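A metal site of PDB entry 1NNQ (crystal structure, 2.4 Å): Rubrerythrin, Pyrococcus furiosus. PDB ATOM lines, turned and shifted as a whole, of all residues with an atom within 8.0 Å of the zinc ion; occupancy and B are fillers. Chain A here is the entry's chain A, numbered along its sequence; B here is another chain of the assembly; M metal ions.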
ATOM      1  N   TYR A 109     -16.066 -22.911  10.247  1.00  0.00           N
ATOM      2  CA  TYR A 109     -14.821 -23.619   9.926  1.00  0.00           C
ATOM      3  C   TYR A 109     -13.820 -22.646   9.282  1.00  0.00           C
ATOM      4  O   TYR A 109     -12.697 -22.542   9.692  1.00  0.00           O
ATOM      5  CB  TYR A 109     -15.106 -24.841   9.036  1.00  0.00           C
ATOM      6  CG  TYR A 109     -15.605 -26.088   9.750  1.00  0.00           C
ATOM      7  CD1 TYR A 109     -15.822 -26.100  11.140  1.00  0.00           C
ATOM      8  CD2 TYR A 109     -15.853 -27.272   9.041  1.00  0.00           C
ATOM      9  CE1 TYR A 109     -16.270 -27.257  11.790  1.00  0.00           C
ATOM     10  CE2 TYR A 109     -16.308 -28.436   9.689  1.00  0.00           C
ATOM     11  CZ  TYR A 109     -16.522 -28.413  11.056  1.00  0.00           C
ATOM     12  OH  TYR A 109     -16.955 -29.554  11.702  1.00  0.00           O
ATOM     13  N   ILE A 141      -2.487 -29.145   7.894  1.00  0.00           N
ATOM     14  CA  ILE A 141      -3.826 -28.662   7.574  1.00  0.00           C
ATOM     15  C   ILE A 141      -4.901 -29.717   7.875  1.00  0.00           C
ATOM     16  O   ILE A 141      -4.841 -30.816   7.336  1.00  0.00           O
ATOM     17  CB  ILE A 141      -3.932 -28.254   6.067  1.00  0.00           C
ATOM     18  CG1 ILE A 141      -2.698 -27.453   5.550  1.00  0.00           C
ATOM     19  CG2 ILE A 141      -5.282 -27.567   5.805  1.00  0.00           C
ATOM     20  CD1 ILE A 141      -2.501 -26.066   6.156  1.00  0.00           C
ATOM     21  N   CYS A 142      -5.895 -29.384   8.693  1.00  0.00           N
ATOM     22  CA  CYS A 142      -7.027 -30.284   8.878  1.00  0.00           C
ATOM     23  C   CYS A 142      -7.868 -30.320   7.591  1.00  0.00           C
ATOM     24  O   CYS A 142      -8.307 -29.267   7.137  1.00  0.00           O
ATOM     25  CB  CYS A 142      -7.881 -29.877  10.088  1.00  0.00           C
ATOM     26  SG  CYS A 142      -9.376 -30.896  10.367  1.00  0.00           S
ATOM     27  N   PRO A 143      -8.060 -31.512   7.023  1.00  0.00           N
ATOM     28  CA  PRO A 143      -8.811 -31.659   5.763  1.00  0.00           C
ATOM     29  C   PRO A 143     -10.323 -31.584   5.963  1.00  0.00           C
ATOM     30  O   PRO A 143     -11.051 -31.639   4.968  1.00  0.00           O
ATOM     31  CB  PRO A 143      -8.390 -33.051   5.279  1.00  0.00           C
ATOM     32  CG  PRO A 143      -8.254 -33.856   6.622  1.00  0.00           C
ATOM     33  CD  PRO A 143      -7.592 -32.819   7.544  1.00  0.00           C
ATOM     34  N   ILE A 144     -10.797 -31.417   7.191  1.00  0.00           N
ATOM     35  CA  ILE A 144     -12.238 -31.242   7.478  1.00  0.00           C
ATOM     36  C   ILE A 144     -12.585 -29.770   7.608  1.00  0.00           C
ATOM     37  O   ILE A 144     -13.553 -29.263   7.016  1.00  0.00           O
ATOM     38  CB  ILE A 144     -12.607 -31.957   8.798  1.00  0.00           C
ATOM     39  CG1 ILE A 144     -12.184 -33.431   8.783  1.00  0.00           C
ATOM     40  CG2 ILE A 144     -14.107 -31.793   9.146  1.00  0.00           C
ATOM     41  CD1 ILE A 144     -12.911 -34.290   7.708  1.00  0.00           C
ATOM     42  N   CYS A 145     -11.799 -29.045   8.400  1.00  0.00           N
ATOM     43  CA  CYS A 145     -12.145 -27.672   8.672  1.00  0.00           C
ATOM     44  C   CYS A 145     -11.090 -26.672   8.229  1.00  0.00           C
ATOM     45  O   CYS A 145     -11.312 -25.475   8.321  1.00  0.00           O
ATOM     46  CB  CYS A 145     -12.443 -27.528  10.160  1.00  0.00           C
ATOM     47  SG  CYS A 145     -10.940 -27.519  11.144  1.00  0.00           S
ATOM     48  N   GLY A 146      -9.928 -27.134   7.779  1.00  0.00           N
ATOM     49  CA  GLY A 146      -8.884 -26.233   7.322  1.00  0.00           C
ATOM     50  C   GLY A 146      -8.030 -25.545   8.375  1.00  0.00           C
ATOM     51  O   GLY A 146      -7.195 -24.688   8.031  1.00  0.00           O
ATOM     52  N   TYR A 147      -8.238 -25.904   9.639  1.00  0.00           N
ATOM     53  CA  TYR A 147      -7.343 -25.530  10.736  1.00  0.00           C
ATOM     54  C   TYR A 147      -5.883 -25.731  10.321  1.00  0.00           C
ATOM     55  O   TYR A 147      -5.531 -26.730   9.694  1.00  0.00           O
ATOM     56  CB  TYR A 147      -7.659 -26.345  11.999  1.00  0.00           C
ATOM     57  CG  TYR A 147      -6.573 -26.278  13.081  1.00  0.00           C
ATOM     58  CD1 TYR A 147      -5.586 -27.269  13.173  1.00  0.00           C
ATOM     59  CD2 TYR A 147      -6.555 -25.215  14.007  1.00  0.00           C
ATOM     60  CE1 TYR A 147      -4.588 -27.203  14.179  1.00  0.00           C
ATOM     61  CE2 TYR A 147      -5.555 -25.131  14.997  1.00  0.00           C
ATOM     62  CZ  TYR A 147      -4.581 -26.134  15.075  1.00  0.00           C
ATOM     63  OH  TYR A 147      -3.607 -26.063  16.057  1.00  0.00           O
ATOM     64  N   THR A 148      -5.039 -24.778  10.709  1.00  0.00           N
ATOM     65  CA  THR A 148      -3.690 -24.664  10.199  1.00  0.00           C
ATOM     66  C   THR A 148      -2.681 -24.540  11.366  1.00  0.00           C
ATOM     67  O   THR A 148      -2.837 -23.689  12.226  1.00  0.00           O
ATOM     68  CB  THR A 148      -3.632 -23.422   9.324  1.00  0.00           C
ATOM     69  OG1 THR A 148      -4.566 -23.560   8.237  1.00  0.00           O
ATOM     70  CG2 THR A 148      -2.274 -23.300   8.661  1.00  0.00           C
ATOM     71  N   TYR A 156      -5.652 -33.456  18.448  1.00  0.00           N
ATOM     72  CA  TYR A 156      -6.970 -33.355  17.841  1.00  0.00           C
ATOM     73  C   TYR A 156      -7.142 -31.941  17.390  1.00  0.00           C
ATOM     74  O   TYR A 156      -6.698 -31.001  18.059  1.00  0.00           O
ATOM     75  CB  TYR A 156      -8.074 -33.747  18.840  1.00  0.00           C
ATOM     76  CG  TYR A 156      -7.988 -35.218  19.202  1.00  0.00           C
ATOM     77  CD1 TYR A 156      -8.631 -36.188  18.434  1.00  0.00           C
ATOM     78  CD2 TYR A 156      -7.204 -35.641  20.297  1.00  0.00           C
ATOM     79  CE1 TYR A 156      -8.537 -37.541  18.732  1.00  0.00           C
ATOM     80  CE2 TYR A 156      -7.091 -37.006  20.616  1.00  0.00           C
ATOM     81  CZ  TYR A 156      -7.759 -37.942  19.821  1.00  0.00           C
ATOM     82  OH  TYR A 156      -7.677 -39.293  20.108  1.00  0.00           O
ATOM     83  N   CYS A 157      -7.777 -31.779  16.233  1.00  0.00           N
ATOM     84  CA  CYS A 157      -8.133 -30.471  15.729  1.00  0.00           C
ATOM     85  C   CYS A 157      -8.998 -29.765  16.750  1.00  0.00           C
ATOM     86  O   CYS A 157     -10.015 -30.294  17.177  1.00  0.00           O
ATOM     87  CB  CYS A 157      -8.889 -30.601  14.400  1.00  0.00           C
ATOM     88  SG  CYS A 157      -9.399 -29.001  13.705  1.00  0.00           S
ATOM     89  N   PRO A 158      -8.599 -28.572  17.172  1.00  0.00           N
ATOM     90  CA  PRO A 158      -9.387 -27.823  18.152  1.00  0.00           C
ATOM     91  C   PRO A 158     -10.725 -27.306  17.591  1.00  0.00           C
ATOM     92  O   PRO A 158     -11.560 -26.844  18.390  1.00  0.00           O
ATOM     93  CB  PRO A 158      -8.486 -26.626  18.473  1.00  0.00           C
ATOM     94  CG  PRO A 158      -7.633 -26.443  17.261  1.00  0.00           C
ATOM     95  CD  PRO A 158      -7.391 -27.850  16.736  1.00  0.00           C
ATOM     96  N   VAL A 159     -10.918 -27.360  16.270  1.00  0.00           N
ATOM     97  CA  VAL A 159     -12.161 -26.827  15.696  1.00  0.00           C
ATOM     98  C   VAL A 159     -13.192 -27.938  15.470  1.00  0.00           C
ATOM     99  O   VAL A 159     -14.327 -27.814  15.914  1.00  0.00           O
ATOM    100  CB  VAL A 159     -11.935 -25.974  14.408  1.00  0.00           C
ATOM    101  CG1 VAL A 159     -13.257 -25.484  13.843  1.00  0.00           C
ATOM    102  CG2 VAL A 159     -11.007 -24.790  14.698  1.00  0.00           C
ATOM    103  N   CYS A 160     -12.764 -29.013  14.815  1.00  0.00           N
ATOM    104  CA  CYS A 160     -13.695 -30.092  14.446  1.00  0.00           C
ATOM    105  C   CYS A 160     -13.461 -31.405  15.190  1.00  0.00           C
ATOM    106  O   CYS A 160     -14.298 -32.316  15.084  1.00  0.00           O
ATOM    107  CB  CYS A 160     -13.641 -30.351  12.935  1.00  0.00           C
ATOM    108  SG  CYS A 160     -12.153 -31.201  12.346  1.00  0.00           S
ATOM    109  N   GLY A 161     -12.346 -31.543  15.915  1.00  0.00           N
ATOM    110  CA  GLY A 161     -12.062 -32.757  16.649  1.00  0.00           C
ATOM    111  C   GLY A 161     -11.337 -33.872  15.883  1.00  0.00           C
ATOM    112  O   GLY A 161     -10.973 -34.857  16.497  1.00  0.00           O
ATOM    113  N   ALA A 162     -11.100 -33.700  14.587  1.00  0.00           N
ATOM    114  CA  ALA A 162     -10.323 -34.667  13.791  1.00  0.00           C
ATOM    115  C   ALA A 162      -8.943 -34.980  14.388  1.00  0.00           C
ATOM    116  O   ALA A 162      -8.295 -34.089  14.939  1.00  0.00           O
ATOM    117  CB  ALA A 162     -10.169 -34.204  12.356  1.00  0.00           C
ATOM    118  N   PRO A 163      -8.501 -36.233  14.273  1.00  0.00           N
ATOM    119  CA  PRO A 163      -7.217 -36.648  14.851  1.00  0.00           C
ATOM    120  C   PRO A 163      -6.051 -36.173  14.006  1.00  0.00           C
ATOM    121  O   PRO A 163      -6.173 -36.114  12.775  1.00  0.00           O
ATOM    122  CB  PRO A 163      -7.280 -38.205  14.837  1.00  0.00           C
ATOM    123  CG  PRO A 163      -8.619 -38.598  14.221  1.00  0.00           C
ATOM    124  CD  PRO A 163      -9.216 -37.349  13.615  1.00  0.00           C
ATOM    125  N   PHE A 167      -4.285 -35.068   9.473  1.00  0.00           N
ATOM    126  CA  PHE A 167      -3.811 -33.791   8.970  1.00  0.00           C
ATOM    127  C   PHE A 167      -2.991 -33.949   7.680  1.00  0.00           C
ATOM    128  O   PHE A 167      -2.238 -34.920   7.514  1.00  0.00           O
ATOM    129  CB  PHE A 167      -3.015 -33.003  10.018  1.00  0.00           C
ATOM    130  CG  PHE A 167      -3.808 -32.620  11.251  1.00  0.00           C
ATOM    131  CD1 PHE A 167      -5.205 -32.810  11.331  1.00  0.00           C
ATOM    132  CD2 PHE A 167      -3.146 -32.086  12.363  1.00  0.00           C
ATOM    133  CE1 PHE A 167      -5.917 -32.464  12.464  1.00  0.00           C
ATOM    134  CE2 PHE A 167      -3.854 -31.723  13.511  1.00  0.00           C
ATOM    135  CZ  PHE A 167      -5.248 -31.921  13.568  1.00  0.00           C
ATOM    136  N   VAL B  54     -10.029 -26.607   1.176  1.00  0.00           N
ATOM    137  CA  VAL B  54     -10.926 -27.243   2.146  1.00  0.00           C
ATOM    138  C   VAL B  54     -12.193 -26.389   2.364  1.00  0.00           C
ATOM    139  O   VAL B  54     -13.304 -26.923   2.329  1.00  0.00           O
ATOM    140  CB  VAL B  54     -10.223 -27.597   3.485  1.00  0.00           C
ATOM    141  CG1 VAL B  54     -11.207 -28.171   4.510  1.00  0.00           C
ATOM    142  CG2 VAL B  54      -9.115 -28.637   3.251  1.00  0.00           C
HETATM  143 ZN    ZN M   1     -10.523 -29.663  11.838  1.00  0.00          ZN
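The backbone NH (N) of Ala 162 lies close to the side-chain sulfur (SG) of Cys 160. SG of Cys 145 sits close to N of Tyr 147 (3.5 Å). The side-chain sulfur (SG) of Cys 157 lies close to the backbone NH (N) of Val 159, at 3.4 Å. O of Tyr 147 lies within hydrogen-bond range of N of Cys 142 (2.9 Å). N of Cys 157 lies within hydrogen-bond range of O of Ala 162 (2.7 Å). The backbone NH of Ile 144 sits close to the side-chain sulfur of Cys 142.
Of the 19 residues printed, 4 come within 4 Å of the zinc ion.
The zinc ion is bound by the side-chain sulfur (SG) of Cys 142 (2.2 Å), the side-chain sulfur (SG) of Cys 157 (2.3 Å), the side-chain sulfur (SG) of Cys 145 (2.3 Å) and the side-chain sulfur (SG) of Cys 160 (2.3 Å). The zinc ion has four donor atoms within binding distance.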
